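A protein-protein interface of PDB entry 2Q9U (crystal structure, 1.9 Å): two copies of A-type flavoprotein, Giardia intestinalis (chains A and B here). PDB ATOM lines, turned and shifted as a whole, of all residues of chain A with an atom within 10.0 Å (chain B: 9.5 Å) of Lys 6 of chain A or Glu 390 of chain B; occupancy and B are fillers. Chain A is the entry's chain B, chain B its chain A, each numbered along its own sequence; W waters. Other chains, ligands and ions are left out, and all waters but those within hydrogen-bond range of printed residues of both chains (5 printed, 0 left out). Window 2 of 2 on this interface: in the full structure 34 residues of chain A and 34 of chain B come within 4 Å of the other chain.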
ATOM      1  N   LYS A   6      11.703  18.389  21.368  1.00  0.00           N
ATOM      2  CA  LYS A   6      11.776  16.950  21.147  1.00  0.00           C
ATOM      3  C   LYS A   6      10.928  16.192  22.163  1.00  0.00           C
ATOM      4  O   LYS A   6      11.240  16.171  23.354  1.00  0.00           O
ATOM      5  CB  LYS A   6      13.228  16.471  21.212  1.00  0.00           C
ATOM      6  CG  LYS A   6      13.457  15.101  20.596  1.00  0.00           C
ATOM      7  CD  LYS A   6      14.849  14.578  20.913  1.00  0.00           C
ATOM      8  CE  LYS A   6      15.132  13.278  20.179  1.00  0.00           C
ATOM      9  NZ  LYS A   6      15.395  13.504  18.731  1.00  0.00           N
ATOM     10  N   TYR A   7       9.854  15.572  21.685  1.00  0.00           N
ATOM     11  CA  TYR A   7       9.050  14.684  22.514  1.00  0.00           C
ATOM     12  C   TYR A   7       8.689  13.406  21.765  1.00  0.00           C
ATOM     13  O   TYR A   7       7.812  12.652  22.189  1.00  0.00           O
ATOM     14  CB  TYR A   7       7.779  15.394  22.986  1.00  0.00           C
ATOM     15  CG  TYR A   7       7.047  16.131  21.888  1.00  0.00           C
ATOM     16  CD1 TYR A   7       6.146  15.472  21.062  1.00  0.00           C
ATOM     17  CD2 TYR A   7       7.257  17.488  21.676  1.00  0.00           C
ATOM     18  CE1 TYR A   7       5.474  16.141  20.058  1.00  0.00           C
ATOM     19  CE2 TYR A   7       6.589  18.166  20.674  1.00  0.00           C
ATOM     20  CZ  TYR A   7       5.700  17.488  19.868  1.00  0.00           C
ATOM     21  OH  TYR A   7       5.033  18.159  18.869  1.00  0.00           O
ATOM     22  N   VAL A   8       9.370  13.168  20.648  1.00  0.00           N
ATOM     23  CA  VAL A   8       9.365  11.856  20.013  1.00  0.00           C
ATOM     24  C   VAL A   8      10.786  11.372  19.740  1.00  0.00           C
ATOM     25  O   VAL A   8      11.698  12.175  19.545  1.00  0.00           O
ATOM     26  CB  VAL A   8       8.575  11.870  18.692  1.00  0.00           C
ATOM     27  CG1 VAL A   8       7.126  12.255  18.945  1.00  0.00           C
ATOM     28  CG2 VAL A   8       9.221  12.825  17.699  1.00  0.00           C
ATOM     29  N   GLN A   9      10.965  10.055  19.727  1.00  0.00           N
ATOM     30  CA  GLN A   9      12.248   9.460  19.371  1.00  0.00           C
ATOM     31  C   GLN A   9      12.241   9.154  17.876  1.00  0.00           C
ATOM     32  O   GLN A   9      11.294   8.521  17.364  1.00  0.00           O
ATOM     33  CB  GLN A   9      12.508   8.166  20.152  1.00  0.00           C
ATOM     34  CG  GLN A   9      13.852   7.496  19.790  1.00  0.00           C
ATOM     35  CD  GLN A   9      13.936   5.988  20.084  1.00  0.00           C
ATOM     36  OE1 GLN A   9      12.981   5.354  20.533  1.00  0.00           O
ATOM     37  NE2 GLN A   9      15.105   5.413  19.818  1.00  0.00           N
ATOM     38  N   ASP A  10      13.280   9.605  17.168  1.00  0.00           N
ATOM     39  CA  ASP A  10      13.432   9.236  15.763  1.00  0.00           C
ATOM     40  C   ASP A  10      13.871   7.796  15.712  1.00  0.00           C
ATOM     41  O   ASP A  10      14.732   7.362  16.498  1.00  0.00           O
ATOM     42  CB  ASP A  10      14.455  10.116  15.028  1.00  0.00           C
ATOM     43  CG  ASP A  10      14.106  11.590  15.090  1.00  0.00           C
ATOM     44  OD1 ASP A  10      12.909  11.949  14.942  1.00  0.00           O
ATOM     45  OD2 ASP A  10      15.043  12.395  15.293  1.00  0.00           O
ATOM     46  N   GLN A  11      13.256   7.049  14.800  1.00  0.00           N
ATOM     47  CA  GLN A  11      13.409   5.613  14.775  1.00  0.00           C
ATOM     48  C   GLN A  11      13.837   5.138  13.386  1.00  0.00           C
ATOM     49  O   GLN A  11      13.018   4.742  12.564  1.00  0.00           O
ATOM     50  CB  GLN A  11      12.122   4.933  15.304  1.00  0.00           C
ATOM     51  CG  GLN A  11      11.884   5.231  16.811  1.00  0.00           C
ATOM     52  CD  GLN A  11      10.507   4.787  17.326  1.00  0.00           C
ATOM     53  OE1 GLN A  11      10.076   3.670  17.079  1.00  0.00           O
ATOM     54  NE2 GLN A  11       9.824   5.675  18.026  1.00  0.00           N
ATOM     55  N   TYR A  18      12.705   5.649   8.112  1.00  0.00           N
ATOM     56  CA  TYR A  18      12.286   5.913   9.487  1.00  0.00           C
ATOM     57  C   TYR A  18      10.844   5.498   9.751  1.00  0.00           C
ATOM     58  O   TYR A  18       9.971   5.703   8.904  1.00  0.00           O
ATOM     59  CB  TYR A  18      12.420   7.396   9.774  1.00  0.00           C
ATOM     60  CG  TYR A  18      13.831   7.881   9.777  1.00  0.00           C
ATOM     61  CD1 TYR A  18      14.523   8.092   8.577  1.00  0.00           C
ATOM     62  CD2 TYR A  18      14.486   8.128  10.983  1.00  0.00           C
ATOM     63  CE1 TYR A  18      15.856   8.546   8.583  1.00  0.00           C
ATOM     64  CE2 TYR A  18      15.788   8.554  11.001  1.00  0.00           C
ATOM     65  CZ  TYR A  18      16.465   8.771   9.804  1.00  0.00           C
ATOM     66  OH  TYR A  18      17.771   9.211   9.844  1.00  0.00           O
ATOM     67  N   SER A  67       3.914  15.039  13.984  1.00  0.00           N
ATOM     68  CA  SER A  67       5.064  15.341  14.836  1.00  0.00           C
ATOM     69  C   SER A  67       6.274  14.483  14.532  1.00  0.00           C
ATOM     70  O   SER A  67       7.411  14.997  14.525  1.00  0.00           O
ATOM     71  CB  SER A  67       4.727  15.221  16.318  1.00  0.00           C
ATOM     72  OG  SER A  67       3.813  16.216  16.678  1.00  0.00           O
ATOM     73  N   ARG A  68       6.053  13.183  14.298  1.00  0.00           N
ATOM     74  CA  ARG A  68       7.173  12.282  13.990  1.00  0.00           C
ATOM     75  C   ARG A  68       7.745  12.587  12.599  1.00  0.00           C
ATOM     76  O   ARG A  68       8.945  12.498  12.385  1.00  0.00           O
ATOM     77  CB  ARG A  68       6.760  10.810  14.071  1.00  0.00           C
ATOM     78  CG  ARG A  68       6.284  10.338  15.441  1.00  0.00           C
ATOM     79  CD  ARG A  68       6.044   8.843  15.386  1.00  0.00           C
ATOM     80  NE  ARG A  68       5.407   8.284  16.575  1.00  0.00           N
ATOM     81  CZ  ARG A  68       6.048   8.034  17.712  1.00  0.00           C
ATOM     82  NH1 ARG A  68       7.343   8.322  17.839  1.00  0.00           N
ATOM     83  NH2 ARG A  68       5.394   7.489  18.735  1.00  0.00           N
ATOM     84  N   ALA A  70       7.664  15.579  11.149  1.00  0.00           N
ATOM     85  CA  ALA A  70       8.302  16.887  11.294  1.00  0.00           C
ATOM     86  C   ALA A  70       9.658  16.758  11.982  1.00  0.00           C
ATOM     87  O   ALA A  70      10.580  17.564  11.749  1.00  0.00           O
ATOM     88  CB  ALA A  70       7.416  17.805  12.088  1.00  0.00           C
ATOM     89  N   ALA A  71       9.778  15.769  12.866  1.00  0.00           N
ATOM     90  CA  ALA A  71      11.056  15.538  13.517  1.00  0.00           C
ATOM     91  C   ALA A  71      12.113  15.097  12.503  1.00  0.00           C
ATOM     92  O   ALA A  71      13.285  15.367  12.713  1.00  0.00           O
ATOM     93  CB  ALA A  71      10.931  14.534  14.698  1.00  0.00           C
ATOM     94  N   CYS A  72      11.688  14.447  11.409  1.00  0.00           N
ATOM     95  CA  CYS A  72      12.572  13.998  10.334  1.00  0.00           C
ATOM     96  C   CYS A  72      12.810  15.052   9.253  1.00  0.00           C
ATOM     97  O   CYS A  72      13.937  15.168   8.723  1.00  0.00           O
ATOM     98  CB  CYS A  72      12.007  12.760   9.634  1.00  0.00           C
ATOM     99  SG  CYS A  72      12.051  11.235  10.637  1.00  0.00           S
ATOM    100  N   ARG B 272      -1.695  11.492  26.535  1.00  0.00           N
ATOM    101  CA  ARG B 272      -0.717  12.066  25.597  1.00  0.00           C
ATOM    102  C   ARG B 272       0.650  12.323  26.263  1.00  0.00           C
ATOM    103  O   ARG B 272       1.697  12.082  25.658  1.00  0.00           O
ATOM    104  CB  ARG B 272      -1.222  13.365  24.969  1.00  0.00           C
ATOM    105  CG  ARG B 272      -0.235  13.986  23.950  1.00  0.00           C
ATOM    106  CD  ARG B 272      -0.221  13.155  22.669  1.00  0.00           C
ATOM    107  NE  ARG B 272       0.846  13.492  21.709  1.00  0.00           N
ATOM    108  CZ  ARG B 272       2.136  13.158  21.823  1.00  0.00           C
ATOM    109  NH1 ARG B 272       2.606  12.524  22.895  1.00  0.00           N
ATOM    110  NH2 ARG B 272       2.971  13.497  20.855  1.00  0.00           N
ATOM    111  N   MET B 273       0.636  12.796  27.500  1.00  0.00           N
ATOM    112  CA  MET B 273       1.896  12.974  28.222  1.00  0.00           C
ATOM    113  C   MET B 273       2.578  11.622  28.438  1.00  0.00           C
ATOM    114  O   MET B 273       3.821  11.514  28.362  1.00  0.00           O
ATOM    115  CB  MET B 273       1.675  13.663  29.548  1.00  0.00           C
ATOM    116  CG  MET B 273       1.255  15.092  29.405  1.00  0.00           C
ATOM    117  SD  MET B 273       2.682  16.119  29.056  1.00  0.00           S
ATOM    118  CE  MET B 273       3.291  16.275  30.745  1.00  0.00           C
ATOM    119  N   LEU B 275       2.454   9.104  26.441  1.00  0.00           N
ATOM    120  CA  LEU B 275       3.111   8.707  25.190  1.00  0.00           C
ATOM    121  C   LEU B 275       4.481   9.388  25.018  1.00  0.00           C
ATOM    122  O   LEU B 275       5.435   8.783  24.526  1.00  0.00           O
ATOM    123  CB  LEU B 275       2.210   9.000  23.970  1.00  0.00           C
ATOM    124  CG  LEU B 275       0.973   8.112  23.766  1.00  0.00           C
ATOM    125  CD1 LEU B 275       0.058   8.727  22.689  1.00  0.00           C
ATOM    126  CD2 LEU B 275       1.395   6.672  23.375  1.00  0.00           C
ATOM    127  N   ALA B 276       4.567  10.665  25.379  1.00  0.00           N
ATOM    128  CA  ALA B 276       5.841  11.398  25.284  1.00  0.00           C
ATOM    129  C   ALA B 276       6.884  10.805  26.244  1.00  0.00           C
ATOM    130  O   ALA B 276       8.054  10.627  25.880  1.00  0.00           O
ATOM    131  CB  ALA B 276       5.634  12.916  25.586  1.00  0.00           C
ATOM    132  N   LEU B 277       6.454  10.523  27.466  1.00  0.00           N
ATOM    133  CA  LEU B 277       7.320   9.870  28.449  1.00  0.00           C
ATOM    134  C   LEU B 277       7.831   8.530  27.909  1.00  0.00           C
ATOM    135  O   LEU B 277       9.003   8.184  28.057  1.00  0.00           O
ATOM    136  CB  LEU B 277       6.586   9.670  29.773  1.00  0.00           C
ATOM    137  CG  LEU B 277       7.459   9.134  30.911  1.00  0.00           C
ATOM    138  CD1 LEU B 277       7.350  10.014  32.132  1.00  0.00           C
ATOM    139  CD2 LEU B 277       7.072   7.737  31.275  1.00  0.00           C
ATOM    140  N   ASP B 279       8.175   7.482  24.766  1.00  0.00           N
ATOM    141  CA  ASP B 279       9.216   7.698  23.759  1.00  0.00           C
ATOM    142  C   ASP B 279      10.565   8.036  24.372  1.00  0.00           C
ATOM    143  O   ASP B 279      11.570   7.563  23.879  1.00  0.00           O
ATOM    144  CB  ASP B 279       8.824   8.722  22.688  1.00  0.00           C
ATOM    145  CG  ASP B 279       8.327   8.055  21.408  1.00  0.00           C
ATOM    146  OD1 ASP B 279       7.573   7.046  21.509  1.00  0.00           O
ATOM    147  OD2 ASP B 279       8.707   8.526  20.305  1.00  0.00           O
ATOM    148  N   GLY B 280      10.574   8.840  25.432  1.00  0.00           N
ATOM    149  CA  GLY B 280      11.808   9.161  26.148  1.00  0.00           C
ATOM    150  C   GLY B 280      12.430   7.868  26.649  1.00  0.00           C
ATOM    151  O   GLY B 280      13.610   7.605  26.435  1.00  0.00           O
ATOM    152  N   SER B 283      13.909   5.706  23.839  1.00  0.00           N
ATOM    153  CA  SER B 283      15.180   6.255  23.302  1.00  0.00           C
ATOM    154  C   SER B 283      16.434   5.702  23.994  1.00  0.00           C
ATOM    155  O   SER B 283      17.526   5.735  23.415  1.00  0.00           O
ATOM    156  CB  SER B 283      15.195   7.780  23.378  1.00  0.00           C
ATOM    157  OG  SER B 283      15.395   8.241  24.719  1.00  0.00           O
ATOM    158  N   ILE B 378       5.276  15.103  37.397  1.00  0.00           N
ATOM    159  CA  ILE B 378       4.872  16.167  36.482  1.00  0.00           C
ATOM    160  C   ILE B 378       3.374  16.334  36.626  1.00  0.00           C
ATOM    161  O   ILE B 378       2.638  15.377  36.503  1.00  0.00           O
ATOM    162  CB  ILE B 378       5.247  15.881  35.006  1.00  0.00           C
ATOM    163  CG1 ILE B 378       6.776  15.862  34.831  1.00  0.00           C
ATOM    164  CG2 ILE B 378       4.591  16.911  34.082  1.00  0.00           C
ATOM    165  CD1 ILE B 378       7.233  15.269  33.535  1.00  0.00           C
ATOM    166  N   TYR B 384      -1.901  19.735  28.087  1.00  0.00           N
ATOM    167  CA  TYR B 384      -0.464  19.706  27.828  1.00  0.00           C
ATOM    168  C   TYR B 384      -0.119  20.784  26.780  1.00  0.00           C
ATOM    169  O   TYR B 384      -1.014  21.330  26.115  1.00  0.00           O
ATOM    170  CB  TYR B 384      -0.027  18.312  27.334  1.00  0.00           C
ATOM    171  CG  TYR B 384      -0.738  17.874  26.077  1.00  0.00           C
ATOM    172  CD1 TYR B 384      -0.284  18.281  24.810  1.00  0.00           C
ATOM    173  CD2 TYR B 384      -1.878  17.066  26.149  1.00  0.00           C
ATOM    174  CE1 TYR B 384      -0.940  17.900  23.663  1.00  0.00           C
ATOM    175  CE2 TYR B 384      -2.540  16.689  25.011  1.00  0.00           C
ATOM    176  CZ  TYR B 384      -2.068  17.110  23.768  1.00  0.00           C
ATOM    177  OH  TYR B 384      -2.721  16.738  22.625  1.00  0.00           O
ATOM    178  N   THR B 385       1.176  21.072  26.658  1.00  0.00           N
ATOM    179  CA  THR B 385       1.740  21.949  25.631  1.00  0.00           C
ATOM    180  C   THR B 385       2.939  21.229  25.065  1.00  0.00           C
ATOM    181  O   THR B 385       3.398  20.268  25.664  1.00  0.00           O
ATOM    182  CB  THR B 385       2.270  23.254  26.238  1.00  0.00           C
ATOM    183  OG1 THR B 385       3.216  22.962  27.276  1.00  0.00           O
ATOM    184  CG2 THR B 385       1.136  24.074  26.808  1.00  0.00           C
ATOM    185  N   GLU B 386       3.457  21.678  23.927  1.00  0.00           N
ATOM    186  CA  GLU B 386       4.741  21.147  23.462  1.00  0.00           C
ATOM    187  C   GLU B 386       5.858  21.160  24.504  1.00  0.00           C
ATOM    188  O   GLU B 386       6.665  20.235  24.543  1.00  0.00           O
ATOM    189  CB  GLU B 386       5.201  21.847  22.201  1.00  0.00           C
ATOM    190  CG  GLU B 386       4.494  21.300  20.976  1.00  0.00           C
ATOM    191  CD  GLU B 386       5.260  21.563  19.715  1.00  0.00           C
ATOM    192  OE1 GLU B 386       5.929  22.614  19.636  1.00  0.00           O
ATOM    193  OE2 GLU B 386       5.204  20.714  18.804  1.00  0.00           O
ATOM    194  N   GLU B 387       5.904  22.195  25.339  1.00  0.00           N
ATOM    195  CA  GLU B 387       6.926  22.284  26.381  1.00  0.00           C
ATOM    196  C   GLU B 387       6.754  21.175  27.418  1.00  0.00           C
ATOM    197  O   GLU B 387       7.747  20.581  27.854  1.00  0.00           O
ATOM    198  CB  GLU B 387       6.903  23.656  27.064  1.00  0.00           C
ATOM    199  N   LEU B 388       5.498  20.928  27.811  1.00  0.00           N
ATOM    200  CA  LEU B 388       5.173  19.855  28.750  1.00  0.00           C
ATOM    201  C   LEU B 388       5.476  18.461  28.183  1.00  0.00           C
ATOM    202  O   LEU B 388       6.008  17.622  28.900  1.00  0.00           O
ATOM    203  CB  LEU B 388       3.724  19.947  29.224  1.00  0.00           C
ATOM    204  CG  LEU B 388       3.448  20.827  30.444  1.00  0.00           C
ATOM    205  CD1 LEU B 388       1.959  21.218  30.469  1.00  0.00           C
ATOM    206  CD2 LEU B 388       3.852  20.153  31.759  1.00  0.00           C
ATOM    207  N   LEU B 389       5.139  18.219  26.919  1.00  0.00           N
ATOM    208  CA  LEU B 389       5.522  16.969  26.246  1.00  0.00           C
ATOM    209  C   LEU B 389       7.054  16.730  26.256  1.00  0.00           C
ATOM    210  O   LEU B 389       7.522  15.606  26.463  1.00  0.00           O
ATOM    211  CB  LEU B 389       5.014  16.963  24.797  1.00  0.00           C
ATOM    212  CG  LEU B 389       3.487  17.018  24.622  1.00  0.00           C
ATOM    213  CD1 LEU B 389       3.142  17.056  23.143  1.00  0.00           C
ATOM    214  CD2 LEU B 389       2.829  15.793  25.288  1.00  0.00           C
ATOM    215  N   GLU B 390       7.817  17.789  26.010  1.00  0.00           N
ATOM    216  CA  GLU B 390       9.274  17.730  26.093  1.00  0.00           C
ATOM    217  C   GLU B 390       9.748  17.377  27.502  1.00  0.00           C
ATOM    218  O   GLU B 390      10.655  16.556  27.673  1.00  0.00           O
ATOM    219  CB  GLU B 390       9.882  19.061  25.640  1.00  0.00           C
ATOM    220  CG  GLU B 390      11.386  19.054  25.709  1.00  0.00           C
ATOM    221  CD  GLU B 390      12.012  20.313  25.158  1.00  0.00           C
ATOM    222  OE1 GLU B 390      11.623  21.410  25.599  1.00  0.00           O
ATOM    223  OE2 GLU B 390      12.901  20.194  24.283  1.00  0.00           O
ATOM    224  N   GLN B 391       9.125  17.981  28.516  1.00  0.00           N
ATOM    225  CA  GLN B 391       9.462  17.672  29.896  1.00  0.00           C
ATOM    226  C   GLN B 391       9.136  16.195  30.203  1.00  0.00           C
ATOM    227  O   GLN B 391       9.892  15.500  30.899  1.00  0.00           O
ATOM    228  CB  GLN B 391       8.726  18.624  30.846  1.00  0.00           C
ATOM    229  CG  GLN B 391       8.977  18.359  32.305  1.00  0.00           C
ATOM    230  CD  GLN B 391       8.265  19.339  33.214  1.00  0.00           C
ATOM    231  OE1 GLN B 391       7.434  20.130  32.763  1.00  0.00           O
ATOM    232  NE2 GLN B 391       8.595  19.300  34.505  1.00  0.00           N
ATOM    233  N   ALA B 392       8.018  15.723  29.653  1.00  0.00           N
ATOM    234  CA  ALA B 392       7.613  14.320  29.839  1.00  0.00           C
ATOM    235  C   ALA B 392       8.612  13.397  29.180  1.00  0.00           C
ATOM    236  O   ALA B 392       9.008  12.396  29.769  1.00  0.00           O
ATOM    237  CB  ALA B 392       6.195  14.079  29.287  1.00  0.00           C
ATOM    238  N   TYR B 393       9.009  13.742  27.959  1.00  0.00           N
ATOM    239  CA  TYR B 393      10.004  12.979  27.190  1.00  0.00           C
ATOM    240  C   TYR B 393      11.308  12.886  27.970  1.00  0.00           C
ATOM    241  O   TYR B 393      11.890  11.800  28.071  1.00  0.00           O
ATOM    242  CB  TYR B 393      10.244  13.606  25.813  1.00  0.00           C
ATOM    243  CG  TYR B 393      11.275  12.895  24.953  1.00  0.00           C
ATOM    244  CD1 TYR B 393      12.653  13.156  25.089  1.00  0.00           C
ATOM    245  CD2 TYR B 393      10.876  11.967  23.999  1.00  0.00           C
ATOM    246  CE1 TYR B 393      13.592  12.486  24.275  1.00  0.00           C
ATOM    247  CE2 TYR B 393      11.794  11.316  23.193  1.00  0.00           C
ATOM    248  CZ  TYR B 393      13.133  11.568  23.327  1.00  0.00           C
ATOM    249  OH  TYR B 393      13.986  10.876  22.483  1.00  0.00           O
ATOM    250  N   ASN B 394      11.763  14.027  28.512  1.00  0.00           N
ATOM    251  CA  ASN B 394      12.993  14.044  29.314  1.00  0.00           C
ATOM    252  C   ASN B 394      12.908  13.213  30.599  1.00  0.00           C
ATOM    253  O   ASN B 394      13.870  12.523  30.967  1.00  0.00           O
ATOM    254  CB  ASN B 394      13.434  15.480  29.633  1.00  0.00           C
ATOM    255  CG  ASN B 394      13.865  16.245  28.387  1.00  0.00           C
ATOM    256  OD1 ASN B 394      14.216  15.654  27.341  1.00  0.00           O
ATOM    257  ND2 ASN B 394      13.811  17.560  28.477  1.00  0.00           N
ATOM    258  N   ALA B 395      11.772  13.299  31.289  1.00  0.00           N
ATOM    259  CA  ALA B 395      11.519  12.448  32.445  1.00  0.00           C
ATOM    260  C   ALA B 395      11.564  10.962  32.060  1.00  0.00           C
ATOM    261  O   ALA B 395      12.018  10.135  32.851  1.00  0.00           O
ATOM    262  CB  ALA B 395      10.214  12.809  33.115  1.00  0.00           C
ATOM    263  N   GLY B 396      11.121  10.640  30.842  1.00  0.00           N
ATOM    264  CA  GLY B 396      11.163   9.264  30.327  1.00  0.00           C
ATOM    265  C   GLY B 396      12.577   8.790  30.033  1.00  0.00           C
ATOM    266  O   GLY B 396      12.938   7.662  30.340  1.00  0.00           O
ATOM    267  N   VAL B 397      13.386   9.656  29.437  1.00  0.00           N
ATOM    268  CA  VAL B 397      14.777   9.312  29.176  1.00  0.00           C
ATOM    269  C   VAL B 397      15.412   8.905  30.502  1.00  0.00           C
ATOM    270  O   VAL B 397      16.067   7.859  30.583  1.00  0.00           O
ATOM    271  CB  VAL B 397      15.586  10.485  28.527  1.00  0.00           C
ATOM    272  CG1 VAL B 397      17.091  10.077  28.326  1.00  0.00           C
ATOM    273  CG2 VAL B 397      15.002  10.879  27.195  1.00  0.00           C
ATOM    274  N   ASP B 398      15.204   9.728  31.537  1.00  0.00           N
ATOM    275  CA  ASP B 398      15.805   9.532  32.852  1.00  0.00           C
ATOM    276  C   ASP B 398      15.269   8.246  33.489  1.00  0.00           C
ATOM    277  O   ASP B 398      16.009   7.501  34.144  1.00  0.00           O
ATOM    278  CB  ASP B 398      15.508  10.739  33.771  1.00  0.00           C
ATOM    279  CG  ASP B 398      15.948  10.503  35.240  1.00  0.00           C
ATOM    280  OD1 ASP B 398      17.165  10.489  35.534  1.00  0.00           O
ATOM    281  OD2 ASP B 398      15.092  10.341  36.117  1.00  0.00           O
HETATM  282  O   HOH W   1       1.838  15.232  18.907  1.00  0.00           O
HETATM  283  O   HOH W   2       5.157  11.887  21.793  1.00  0.00           O
HETATM  284  O   HOH W   3      13.589  16.499  24.967  1.00  0.00           O
HETATM  285  O   HOH W   4       7.288   5.355  19.584  1.00  0.00           O
HETATM  286  O   HOH W   5       4.566   9.356  21.250  1.00  0.00           O
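No position is printed for both chains.
The backbone carbonyl oxygen of Gln 9 of chain A sits at hydrogen-bond distance from the side-chain amide nitrogen of Gln 11 of chain A (3.3 Å). NZ of Lys 6 of chain A is in salt-bridge range of OD2 of Asp 10 of chain A. The side-chain hydroxyl of Ser 67 of chain A lies within hydrogen-bond range of the side-chain hydroxyl of Tyr 7 of chain A (3.2 Å). ND2 of Asn 394 of chain B lies close to O of Glu 390 of chain B (3.4 Å). The backbone carbonyl oxygen of Arg 68 of chain A lies within hydrogen-bond range of the side-chain sulfur of Cys 72 of chain A, at 3.8 Å. The backbone carbonyl oxygen of Gly 280 of chain B is in hydrogen-bond range of the side-chain hydroxyl of Ser 283 of chain B, at 2.6 Å.
Of the 24 printed residues of chain B, 8 touch a printed residue of chain A. Printed residues of chain B that touch a printed residue of chain A: Arg 272, Ala 276, Asp 279, Ser 283, Glu 386, Leu 389, Glu 390 and Tyr 393. Hydrophobic or aromatic side chains of chain B that line the printed part of chain A: Leu 389 and Tyr 393.
Water W4 lies within hydrogen-bond range of the side-chain carboxylate of Asp 279 of chain B (2.6 Å), the guanidinium group of Arg 68 of chain A (3.0 Å) and the side-chain amide nitrogen of Gln 11 of chain A (3.0 Å). Water W3 lies within hydrogen-bond range of OD1 of Asn 394 of chain B (2.6 Å) and O of Lys 6 of chain A (2.9 Å). Water W2 bridges the backbone carbonyl oxygen (O) of Tyr 7 of chain A and the guanidinium group (NH1) of Arg 272 of chain B. Water W1 lies within hydrogen-bond range of NH2 of Arg 272 of chain B and OG of Ser 67 of chain A. Water W5 lies within hydrogen-bond range of NH2 of Arg 68 of chain A (3.2 Å) and O of Leu 275 of chain B (3.4 Å).
Among the printed residues, pairs that only touch across the chains: Lys 6 of chain A with Glu 390 of chain B (3.6 Å), Lys 6 of chain A with Tyr 393 of chain B (3.5 Å), Tyr 7 of chain A with Arg 272 of chain B (3.7 Å), Tyr 7 of chain A with Ala 276 of chain B (3.9 Å), Tyr 7 of chain A with Leu 389 of chain B (3.5 Å), Tyr 7 of chain A with Glu 390 of chain B (3.9 Å), Tyr 7 of chain A with Tyr 393 of chain B (3.4 Å), Val 8 of chain A with Asp 279 of chain B (3.4 Å), Val 8 of chain A with Tyr 393 of chain B (3.6 Å), Gln 9 of chain A with Tyr 393 of chain B (3.8 Å) and Gln 11 of chain A with Asp 279 of chain B (3.8 Å).
Of chain B, only Glu 390 (3.6 Å) and Tyr 393 (3.5 Å) come within 4 Å of Lys 6 of chain A. Of the printed residues of chain A, Arg 272 of chain B touches Tyr 7 (3.7 Å). Of the printed residues of chain A, Ser 283 of chain B touches Gln 9 (3.5 Å). No residue of chain A comes within 4 Å of Glu 387 of chain B. Of the printed residues of chain A, Glu 390 of chain B touches Lys 6 and Tyr 7. No residue of chain A comes within 4 Å of Ala 392 of chain B. Printed residues of chain A within 4 Å of Tyr 393 of chain B: Lys 6 (3.5 Å), Tyr 7 (3.4 Å), Val 8 (3.6 Å) and Gln 9 (3.8 Å).
OE2 of Glu 386 of chain B is in hydrogen-bond range of OH of Tyr 7 of chain A (2.6 Å). The side-chain carboxylate (OD2) of Asp 279 of chain B is in salt-bridge range of the guanidinium group (NH1) of Arg 68 of chain A (2.8 Å). OD2 of Asp 279 of chain B lies within hydrogen-bond range of N of Gln 9 of chain A. The side-chain amide oxygen (OE1) of Gln 9 of chain A sits at hydrogen-bond distance from the backbone NH (N) of Ser 283 of chain B, 3.5 Å away.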
